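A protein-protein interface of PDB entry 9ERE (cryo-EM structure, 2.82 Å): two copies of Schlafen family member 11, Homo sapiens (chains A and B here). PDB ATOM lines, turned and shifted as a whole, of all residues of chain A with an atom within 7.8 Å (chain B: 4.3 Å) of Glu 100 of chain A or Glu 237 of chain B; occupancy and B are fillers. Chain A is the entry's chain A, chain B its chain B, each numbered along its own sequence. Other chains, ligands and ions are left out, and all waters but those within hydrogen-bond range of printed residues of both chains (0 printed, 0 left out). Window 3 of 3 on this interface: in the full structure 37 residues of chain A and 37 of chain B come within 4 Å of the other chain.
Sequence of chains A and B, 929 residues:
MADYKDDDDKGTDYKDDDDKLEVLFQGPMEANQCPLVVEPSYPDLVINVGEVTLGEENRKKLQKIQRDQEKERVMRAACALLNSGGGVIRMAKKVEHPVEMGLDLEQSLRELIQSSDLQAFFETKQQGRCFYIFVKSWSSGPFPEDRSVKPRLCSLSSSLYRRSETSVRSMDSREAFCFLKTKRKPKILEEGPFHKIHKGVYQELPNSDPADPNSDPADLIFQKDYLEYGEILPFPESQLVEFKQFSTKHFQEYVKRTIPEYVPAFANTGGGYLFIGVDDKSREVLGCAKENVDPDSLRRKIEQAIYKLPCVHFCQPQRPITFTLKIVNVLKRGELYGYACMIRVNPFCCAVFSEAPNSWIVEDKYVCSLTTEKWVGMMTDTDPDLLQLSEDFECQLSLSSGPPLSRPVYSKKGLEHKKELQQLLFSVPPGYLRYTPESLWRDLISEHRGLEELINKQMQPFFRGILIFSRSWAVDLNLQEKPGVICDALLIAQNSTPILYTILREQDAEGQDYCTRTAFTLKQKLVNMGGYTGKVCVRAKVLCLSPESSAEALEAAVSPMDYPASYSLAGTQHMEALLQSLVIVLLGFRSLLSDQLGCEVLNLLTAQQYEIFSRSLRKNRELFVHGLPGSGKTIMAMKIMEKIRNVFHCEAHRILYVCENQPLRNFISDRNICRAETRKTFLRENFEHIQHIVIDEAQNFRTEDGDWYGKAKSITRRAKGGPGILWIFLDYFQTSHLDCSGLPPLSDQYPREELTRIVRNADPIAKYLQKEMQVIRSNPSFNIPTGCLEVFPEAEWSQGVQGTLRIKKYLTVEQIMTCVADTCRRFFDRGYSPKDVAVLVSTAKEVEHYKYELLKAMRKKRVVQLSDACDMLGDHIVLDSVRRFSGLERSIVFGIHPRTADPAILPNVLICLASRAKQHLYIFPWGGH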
ATOM      1  N   THR A  53       6.265  16.193  22.407  1.00  0.00           N
ATOM      2  CA  THR A  53       6.174  17.241  21.400  1.00  0.00           C
ATOM      3  C   THR A  53       7.363  17.123  20.458  1.00  0.00           C
ATOM      4  O   THR A  53       8.514  17.249  20.884  1.00  0.00           O
ATOM      5  CB  THR A  53       6.149  18.619  22.051  1.00  0.00           C
ATOM      6  OG1 THR A  53       5.250  18.613  23.164  1.00  0.00           O
ATOM      7  CG2 THR A  53       5.696  19.662  21.056  1.00  0.00           C
ATOM      8  N   LEU A  54       7.084  16.882  19.184  1.00  0.00           N
ATOM      9  CA  LEU A  54       8.112  16.669  18.184  1.00  0.00           C
ATOM     10  C   LEU A  54       8.044  17.781  17.150  1.00  0.00           C
ATOM     11  O   LEU A  54       6.994  18.394  16.942  1.00  0.00           O
ATOM     12  CB  LEU A  54       7.947  15.306  17.511  1.00  0.00           C
ATOM     13  CG  LEU A  54       8.101  14.106  18.442  1.00  0.00           C
ATOM     14  CD1 LEU A  54       7.654  12.857  17.736  1.00  0.00           C
ATOM     15  CD2 LEU A  54       9.531  13.959  18.921  1.00  0.00           C
ATOM     16  N   GLY A  55       9.167  18.032  16.508  1.00  0.00           N
ATOM     17  CA  GLY A  55       9.289  19.169  15.625  1.00  0.00           C
ATOM     18  C   GLY A  55       9.983  20.325  16.313  1.00  0.00           C
ATOM     19  O   GLY A  55       9.726  20.638  17.480  1.00  0.00           O
ATOM     20  N   GLU A  56      10.891  20.968  15.584  1.00  0.00           N
ATOM     21  CA  GLU A  56      11.695  22.018  16.194  1.00  0.00           C
ATOM     22  C   GLU A  56      10.847  23.217  16.597  1.00  0.00           C
ATOM     23  O   GLU A  56      11.000  23.738  17.706  1.00  0.00           O
ATOM     24  CB  GLU A  56      12.814  22.439  15.241  1.00  0.00           C
ATOM     25  CG  GLU A  56      13.760  23.484  15.809  1.00  0.00           C
ATOM     26  CD  GLU A  56      14.316  23.108  17.169  1.00  0.00           C
ATOM     27  OE1 GLU A  56      14.306  21.909  17.513  1.00  0.00           O
ATOM     28  OE2 GLU A  56      14.769  24.016  17.895  1.00  0.00           O
ATOM     29  N   GLU A  57       9.945  23.665  15.724  1.00  0.00           N
ATOM     30  CA  GLU A  57       9.086  24.791  16.078  1.00  0.00           C
ATOM     31  C   GLU A  57       8.191  24.450  17.263  1.00  0.00           C
ATOM     32  O   GLU A  57       8.060  25.244  18.204  1.00  0.00           O
ATOM     33  CB  GLU A  57       8.243  25.200  14.871  1.00  0.00           C
ATOM     34  CG  GLU A  57       9.043  25.823  13.737  1.00  0.00           C
ATOM     35  CD  GLU A  57       9.672  27.150  14.121  1.00  0.00           C
ATOM     36  OE1 GLU A  57       8.971  27.993  14.720  1.00  0.00           O
ATOM     37  OE2 GLU A  57      10.869  27.349  13.825  1.00  0.00           O
ATOM     38  N   ASN A  58       7.580  23.265  17.241  1.00  0.00           N
ATOM     39  CA  ASN A  58       6.687  22.869  18.323  1.00  0.00           C
ATOM     40  C   ASN A  58       7.428  22.806  19.651  1.00  0.00           C
ATOM     41  O   ASN A  58       6.898  23.226  20.684  1.00  0.00           O
ATOM     42  CB  ASN A  58       6.054  21.519  18.001  1.00  0.00           C
ATOM     43  CG  ASN A  58       5.271  21.540  16.713  1.00  0.00           C
ATOM     44  OD1 ASN A  58       4.663  22.549  16.361  1.00  0.00           O
ATOM     45  ND2 ASN A  58       5.282  20.425  15.995  1.00  0.00           N
ATOM     46  N   ARG A  59       8.651  22.276  19.645  1.00  0.00           N
ATOM     47  CA  ARG A  59       9.414  22.190  20.884  1.00  0.00           C
ATOM     48  C   ARG A  59       9.944  23.551  21.312  1.00  0.00           C
ATOM     49  O   ARG A  59      10.194  23.767  22.502  1.00  0.00           O
ATOM     50  CB  ARG A  59      10.560  21.199  20.722  1.00  0.00           C
ATOM     51  CG  ARG A  59      10.100  19.762  20.629  1.00  0.00           C
ATOM     52  CD  ARG A  59      11.265  18.805  20.599  1.00  0.00           C
ATOM     53  NE  ARG A  59      11.961  18.749  21.878  1.00  0.00           N
ATOM     54  CZ  ARG A  59      11.463  18.209  22.981  1.00  0.00           C
ATOM     55  NH1 ARG A  59      10.258  17.669  23.004  1.00  0.00           N
ATOM     56  NH2 ARG A  59      12.198  18.206  24.088  1.00  0.00           N
ATOM     57  N   LYS A  93       2.587  11.504  19.088  1.00  0.00           N
ATOM     58  CA  LYS A  93       2.816  12.882  18.694  1.00  0.00           C
ATOM     59  C   LYS A  93       1.479  13.573  18.482  1.00  0.00           C
ATOM     60  O   LYS A  93       0.510  12.965  18.021  1.00  0.00           O
ATOM     61  CB  LYS A  93       3.682  12.967  17.434  1.00  0.00           C
ATOM     62  CG  LYS A  93       3.171  12.188  16.250  1.00  0.00           C
ATOM     63  CD  LYS A  93       3.978  12.522  15.014  1.00  0.00           C
ATOM     64  CE  LYS A  93       3.365  11.921  13.778  1.00  0.00           C
ATOM     65  NZ  LYS A  93       4.018  12.421  12.550  1.00  0.00           N
ATOM     66  N   HIS A  97       0.732  15.265  10.635  1.00  0.00           N
ATOM     67  CA  HIS A  97       1.685  15.293   9.538  1.00  0.00           C
ATOM     68  C   HIS A  97       3.076  14.876  10.003  1.00  0.00           C
ATOM     69  O   HIS A  97       3.395  14.956  11.190  1.00  0.00           O
ATOM     70  CB  HIS A  97       1.732  16.688   8.923  1.00  0.00           C
ATOM     71  CG  HIS A  97       2.175  17.758   9.873  1.00  0.00           C
ATOM     72  ND1 HIS A  97       3.439  17.796  10.418  1.00  0.00           N
ATOM     73  CD2 HIS A  97       1.516  18.827  10.378  1.00  0.00           C
ATOM     74  CE1 HIS A  97       3.542  18.845  11.215  1.00  0.00           C
ATOM     75  NE2 HIS A  97       2.388  19.486  11.208  1.00  0.00           N
ATOM     76  N   PRO A  98       3.926  14.426   9.080  1.00  0.00           N
ATOM     77  CA  PRO A  98       5.282  14.025   9.469  1.00  0.00           C
ATOM     78  C   PRO A  98       6.047  15.192  10.072  1.00  0.00           C
ATOM     79  O   PRO A  98       5.931  16.333   9.624  1.00  0.00           O
ATOM     80  CB  PRO A  98       5.908  13.567   8.149  1.00  0.00           C
ATOM     81  CG  PRO A  98       4.761  13.260   7.262  1.00  0.00           C
ATOM     82  CD  PRO A  98       3.698  14.237   7.640  1.00  0.00           C
ATOM     83  N   VAL A  99       6.849  14.894  11.090  1.00  0.00           N
ATOM     84  CA  VAL A  99       7.612  15.911  11.798  1.00  0.00           C
ATOM     85  C   VAL A  99       9.048  15.442  11.952  1.00  0.00           C
ATOM     86  O   VAL A  99       9.328  14.242  12.034  1.00  0.00           O
ATOM     87  CB  VAL A  99       7.011  16.226  13.184  1.00  0.00           C
ATOM     88  CG1 VAL A  99       5.617  16.789  13.039  1.00  0.00           C
ATOM     89  CG2 VAL A  99       7.013  14.990  14.063  1.00  0.00           C
ATOM     90  N   GLU A 100       9.963  16.404  11.978  1.00  0.00           N
ATOM     91  CA  GLU A 100      11.323  16.122  12.398  1.00  0.00           C
ATOM     92  C   GLU A 100      11.356  15.890  13.906  1.00  0.00           C
ATOM     93  O   GLU A 100      10.491  16.352  14.654  1.00  0.00           O
ATOM     94  CB  GLU A 100      12.259  17.268  12.005  1.00  0.00           C
ATOM     95  CG  GLU A 100      12.013  18.595  12.723  1.00  0.00           C
ATOM     96  CD  GLU A 100      10.787  19.331  12.219  1.00  0.00           C
ATOM     97  OE1 GLU A 100      10.154  18.847  11.260  1.00  0.00           O
ATOM     98  OE2 GLU A 100      10.457  20.394  12.783  1.00  0.00           O
ATOM     99  N   MET A 101      12.369  15.152  14.353  1.00  0.00           N
ATOM    100  CA  MET A 101      12.460  14.816  15.768  1.00  0.00           C
ATOM    101  C   MET A 101      12.645  16.053  16.636  1.00  0.00           C
ATOM    102  O   MET A 101      12.014  16.166  17.692  1.00  0.00           O
ATOM    103  CB  MET A 101      13.614  13.843  15.991  1.00  0.00           C
ATOM    104  CG  MET A 101      13.555  13.106  17.310  1.00  0.00           C
ATOM    105  SD  MET A 101      14.714  11.729  17.438  1.00  0.00           S
ATOM    106  CE  MET A 101      15.884  12.092  16.132  1.00  0.00           C
ATOM    107  N   GLY A 102      13.492  16.984  16.215  1.00  0.00           N
ATOM    108  CA  GLY A 102      13.827  18.134  17.029  1.00  0.00           C
ATOM    109  C   GLY A 102      15.309  18.184  17.325  1.00  0.00           C
ATOM    110  O   GLY A 102      15.920  17.157  17.629  1.00  0.00           O
ATOM    111  N   LEU A 103      15.897  19.376  17.244  1.00  0.00           N
ATOM    112  CA  LEU A 103      17.342  19.506  17.379  1.00  0.00           C
ATOM    113  C   LEU A 103      17.837  19.140  18.770  1.00  0.00           C
ATOM    114  O   LEU A 103      18.900  18.528  18.894  1.00  0.00           O
ATOM    115  CB  LEU A 103      17.773  20.931  17.037  1.00  0.00           C
ATOM    116  CG  LEU A 103      17.427  21.390  15.623  1.00  0.00           C
ATOM    117  CD1 LEU A 103      17.838  22.829  15.434  1.00  0.00           C
ATOM    118  CD2 LEU A 103      18.089  20.502  14.585  1.00  0.00           C
ATOM    119  N   LEU A 105      16.490  16.992  20.910  1.00  0.00           N
ATOM    120  CA  LEU A 105      16.433  15.539  21.012  1.00  0.00           C
ATOM    121  C   LEU A 105      17.556  14.894  20.208  1.00  0.00           C
ATOM    122  O   LEU A 105      18.202  13.944  20.672  1.00  0.00           O
ATOM    123  CB  LEU A 105      15.068  15.044  20.536  1.00  0.00           C
ATOM    124  CG  LEU A 105      13.909  15.233  21.517  1.00  0.00           C
ATOM    125  CD1 LEU A 105      12.582  15.015  20.822  1.00  0.00           C
ATOM    126  CD2 LEU A 105      14.037  14.291  22.688  1.00  0.00           C
ATOM    127  N   GLU A 106      17.812  15.406  19.003  1.00  0.00           N
ATOM    128  CA  GLU A 106      18.905  14.888  18.188  1.00  0.00           C
ATOM    129  C   GLU A 106      20.239  15.033  18.903  1.00  0.00           C
ATOM    130  O   GLU A 106      21.051  14.104  18.927  1.00  0.00           O
ATOM    131  CB  GLU A 106      18.952  15.625  16.854  1.00  0.00           C
ATOM    132  CG  GLU A 106      17.859  15.268  15.892  1.00  0.00           C
ATOM    133  CD  GLU A 106      17.966  16.058  14.609  1.00  0.00           C
ATOM    134  OE1 GLU A 106      18.988  16.747  14.420  1.00  0.00           O
ATOM    135  OE2 GLU A 106      17.023  16.004  13.795  1.00  0.00           O
ATOM    136  N   THR A 124      14.116   6.521  12.733  1.00  0.00           N
ATOM    137  CA  THR A 124      12.800   6.958  13.161  1.00  0.00           C
ATOM    138  C   THR A 124      11.774   6.692  12.071  1.00  0.00           C
ATOM    139  O   THR A 124      12.032   6.931  10.889  1.00  0.00           O
ATOM    140  CB  THR A 124      12.847   8.456  13.476  1.00  0.00           C
ATOM    141  OG1 THR A 124      12.950   9.202  12.260  1.00  0.00           O
ATOM    142  CG2 THR A 124      14.036   8.779  14.360  1.00  0.00           C
ATOM    143  N   GLN A 126       7.274   7.068  11.509  1.00  0.00           N
ATOM    144  CA  GLN A 126       6.055   7.637  12.058  1.00  0.00           C
ATOM    145  C   GLN A 126       4.896   7.341  11.126  1.00  0.00           C
ATOM    146  O   GLN A 126       4.987   7.565   9.917  1.00  0.00           O
ATOM    147  CB  GLN A 126       6.184   9.145  12.274  1.00  0.00           C
ATOM    148  CG  GLN A 126       6.739   9.908  11.093  1.00  0.00           C
ATOM    149  CD  GLN A 126       7.280  11.257  11.491  1.00  0.00           C
ATOM    150  OE1 GLN A 126       6.637  12.000  12.224  1.00  0.00           O
ATOM    151  NE2 GLN A 126       8.467  11.586  11.006  1.00  0.00           N
ATOM    152  N   PHE A 131       5.053   8.064  16.657  1.00  0.00           N
ATOM    153  CA  PHE A 131       6.425   8.295  16.230  1.00  0.00           C
ATOM    154  C   PHE A 131       7.315   7.251  16.884  1.00  0.00           C
ATOM    155  O   PHE A 131       7.362   7.155  18.113  1.00  0.00           O
ATOM    156  CB  PHE A 131       6.868   9.710  16.613  1.00  0.00           C
ATOM    157  CG  PHE A 131       8.233  10.085  16.117  1.00  0.00           C
ATOM    158  CD1 PHE A 131       9.364   9.756  16.837  1.00  0.00           C
ATOM    159  CD2 PHE A 131       8.381  10.791  14.942  1.00  0.00           C
ATOM    160  CE1 PHE A 131      10.611  10.107  16.383  1.00  0.00           C
ATOM    161  CE2 PHE A 131       9.628  11.144  14.489  1.00  0.00           C
ATOM    162  CZ  PHE A 131      10.743  10.804  15.212  1.00  0.00           C
ATOM    163  N   THR B 166      18.727  15.799  10.830  1.00  0.00           N
ATOM    164  CA  THR B 166      18.413  17.037  10.127  1.00  0.00           C
ATOM    165  C   THR B 166      19.524  18.068  10.210  1.00  0.00           C
ATOM    166  O   THR B 166      19.306  19.215   9.814  1.00  0.00           O
ATOM    167  CB  THR B 166      17.120  17.648  10.667  1.00  0.00           C
ATOM    168  OG1 THR B 166      17.306  18.047  12.029  1.00  0.00           O
ATOM    169  CG2 THR B 166      15.984  16.655  10.585  1.00  0.00           C
ATOM    170  N   PRO B 236       9.297  16.246   6.002  1.00  0.00           N
ATOM    171  CA  PRO B 236      10.142  17.199   6.718  1.00  0.00           C
ATOM    172  C   PRO B 236      11.604  17.042   6.328  1.00  0.00           C
ATOM    173  O   PRO B 236      11.992  16.124   5.607  1.00  0.00           O
ATOM    174  CB  PRO B 236       9.917  16.802   8.172  1.00  0.00           C
ATOM    175  CG  PRO B 236       9.805  15.314   8.095  1.00  0.00           C
ATOM    176  CD  PRO B 236       9.158  14.993   6.761  1.00  0.00           C
ATOM    177  N   GLU B 237      12.421  17.959   6.831  1.00  0.00           N
ATOM    178  CA  GLU B 237      13.858  17.763   6.764  1.00  0.00           C
ATOM    179  C   GLU B 237      14.233  16.520   7.556  1.00  0.00           C
ATOM    180  O   GLU B 237      13.745  16.296   8.666  1.00  0.00           O
ATOM    181  CB  GLU B 237      14.592  18.979   7.319  1.00  0.00           C
ATOM    182  CG  GLU B 237      14.437  20.220   6.478  1.00  0.00           C
ATOM    183  CD  GLU B 237      15.448  21.281   6.833  1.00  0.00           C
ATOM    184  OE1 GLU B 237      15.970  21.243   7.964  1.00  0.00           O
ATOM    185  OE2 GLU B 237      15.726  22.151   5.984  1.00  0.00           O
ATOM    186  N   SER B 238      15.101  15.699   6.980  1.00  0.00           N
ATOM    187  CA  SER B 238      15.441  14.425   7.589  1.00  0.00           C
ATOM    188  C   SER B 238      16.892  14.100   7.264  1.00  0.00           C
ATOM    189  O   SER B 238      17.660  14.964   6.835  1.00  0.00           O
ATOM    190  CB  SER B 238      14.481  13.330   7.110  1.00  0.00           C
ATOM    191  OG  SER B 238      14.754  12.956   5.774  1.00  0.00           O
ATOM    192  N   VAL B 241      17.075  14.797   3.466  1.00  0.00           N
ATOM    193  CA  VAL B 241      16.449  15.983   2.892  1.00  0.00           C
ATOM    194  C   VAL B 241      16.928  17.210   3.647  1.00  0.00           C
ATOM    195  O   VAL B 241      17.133  17.158   4.863  1.00  0.00           O
ATOM    196  CB  VAL B 241      14.912  15.898   2.939  1.00  0.00           C
ATOM    197  CG1 VAL B 241      14.302  17.211   2.507  1.00  0.00           C
ATOM    198  CG2 VAL B 241      14.415  14.767   2.068  1.00  0.00           C
ATOM    199  N   GLU B 242      17.118  18.310   2.924  1.00  0.00           N
ATOM    200  CA  GLU B 242      17.396  19.611   3.511  1.00  0.00           C
ATOM    201  C   GLU B 242      16.665  20.677   2.711  1.00  0.00           C
ATOM    202  O   GLU B 242      16.659  20.644   1.480  1.00  0.00           O
ATOM    203  CB  GLU B 242      18.897  19.912   3.534  1.00  0.00           C
ATOM    204  CG  GLU B 242      19.247  21.260   4.128  1.00  0.00           C
ATOM    205  CD  GLU B 242      18.979  21.325   5.610  1.00  0.00           C
ATOM    206  OE1 GLU B 242      19.222  20.316   6.301  1.00  0.00           O
ATOM    207  OE2 GLU B 242      18.513  22.380   6.088  1.00  0.00           O
ATOM    208  N   PHE B 243      16.048  21.618   3.419  1.00  0.00           N
ATOM    209  CA  PHE B 243      15.353  22.744   2.814  1.00  0.00           C
ATOM    210  C   PHE B 243      16.160  24.008   3.054  1.00  0.00           C
ATOM    211  O   PHE B 243      16.652  24.228   4.165  1.00  0.00           O
ATOM    212  CB  PHE B 243      13.951  22.915   3.401  1.00  0.00           C
ATOM    213  CG  PHE B 243      13.068  21.718   3.237  1.00  0.00           C
ATOM    214  CD1 PHE B 243      13.151  20.926   2.112  1.00  0.00           C
ATOM    215  CD2 PHE B 243      12.145  21.392   4.208  1.00  0.00           C
ATOM    216  CE1 PHE B 243      12.338  19.833   1.964  1.00  0.00           C
ATOM    217  CE2 PHE B 243      11.331  20.299   4.062  1.00  0.00           C
ATOM    218  CZ  PHE B 243      11.426  19.519   2.937  1.00  0.00           C
ATOM    219  N   ASP B 280      11.956  26.780   5.259  1.00  0.00           N
ATOM    220  CA  ASP B 280      12.366  25.736   6.190  1.00  0.00           C
ATOM    221  C   ASP B 280      11.282  25.440   7.220  1.00  0.00           C
ATOM    222  O   ASP B 280      11.140  24.293   7.656  1.00  0.00           O
ATOM    223  CB  ASP B 280      13.665  26.143   6.882  1.00  0.00           C
ATOM    224  CG  ASP B 280      14.272  25.020   7.691  1.00  0.00           C
ATOM    225  OD1 ASP B 280      13.760  24.735   8.792  1.00  0.00           O
ATOM    226  OD2 ASP B 280      15.267  24.424   7.224  1.00  0.00           O
ATOM    227  N   ARG B 283       7.648  24.690   5.010  1.00  0.00           N
ATOM    228  CA  ARG B 283       7.888  23.747   3.922  1.00  0.00           C
ATOM    229  C   ARG B 283       7.294  24.218   2.603  1.00  0.00           C
ATOM    230  O   ARG B 283       7.154  23.413   1.676  1.00  0.00           O
ATOM    231  CB  ARG B 283       7.341  22.353   4.246  1.00  0.00           C
ATOM    232  CG  ARG B 283       7.812  21.797   5.575  1.00  0.00           C
ATOM    233  CD  ARG B 283       7.195  20.439   5.856  1.00  0.00           C
ATOM    234  NE  ARG B 283       7.446  20.005   7.225  1.00  0.00           N
ATOM    235  CZ  ARG B 283       6.853  18.970   7.806  1.00  0.00           C
ATOM    236  NH1 ARG B 283       5.981  18.219   7.156  1.00  0.00           N
ATOM    237  NH2 ARG B 283       7.144  18.683   9.070  1.00  0.00           N
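The guanidinium group (NH2) of Arg 283 of chain B is in hydrogen-bond range of the backbone carbonyl oxygen (O) of Pro 98 of chain A (2.7 Å). The side-chain carboxylate of Glu 100 of chain A lies within salt-bridge range of the guanidinium group of Arg 283 of chain B, 3.7 Å away. The side-chain hydroxyl (OG1) of Thr 166 of chain B sits at hydrogen-bond distance from the side-chain carboxylate (OE2) of Glu 106 of chain A (2.7 Å).
His 97 of chain A touches none of the printed residues of chain B. Of the printed residues of chain B, Val 99 of chain A touches Pro 236 (3.9 Å) and Arg 283 (3.9 Å). Glu 100 of chain A touches just these residues of chain B: Pro 236, Glu 237 and Arg 283. Printed residues of chain B within 4 Å of Leu 103 of chain A: Thr 166 (3.6 Å). Printed residues of chain A within 4 Å of Thr 166 of chain B: Leu 103 (3.6 Å) and Glu 106 (2.7 Å). Phe 243 of chain B touches none of the printed residues of chain A. The nearest residue of chain B that does not touch Glu 100 of chain A is Thr 166 of chain B (4.03 Å). The nearest residue of chain A that does not touch Glu 237 of chain B is Val 99 of chain A (5.8 Å).
Pro 236 of chain B touches Pro 98 of chain A (CD to CB, 3.8 Å). Pro 236 of chain B touches Val 99 of chain A. NH2 of Arg 283 of chain B touches CA of Val 99 of chain A, 3.9 Å away. Glu 100 of chain A touches Pro 236 of chain B. O of Glu 237 of chain B touches CB of Glu 100 of chain A, at 3.8 Å. Leu 103 of chain A touches Thr 166 of chain B (CD2 to OG1, 3.6 Å).
No position is printed for both chains. Of the 9 pairs that touch across the chains among the printed residues, none has its exchanged pair printed and touching as well.
The backbone carbonyl oxygen (O) of Glu 100 of chain A sits at hydrogen-bond distance from the backbone NH (N) of Gly 55 of chain A (2.8 Å). The side-chain carboxylate (OE2) of Glu 100 of chain A sits at hydrogen-bond distance from the backbone NH (N) of Glu 56 of chain A (2.9 Å). The side-chain carboxylate of Glu 56 of chain A lies within hydrogen-bond range of the backbone NH of Leu 103 of chain A (3.0 Å). The backbone carbonyl oxygen (O) of Val 99 of chain A is in hydrogen-bond range of the side-chain amide nitrogen (NE2) of Gln 126 of chain A, 3.0 Å away.
Hydrophobic or aromatic side chains of chain B within 4 Å of the printed part of chain A: Pro 236. Printed residues of chain A that touch a printed residue of chain B: Pro 98, Val 99, Glu 100, Leu 103 and Glu 106. Among the printed residues, Asp or Glu carboxylates within 4 Å of a Lys or Arg side-chain nitrogen of the other chain: Glu 100 of chain A with Arg 283 of chain B (3.7 Å).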
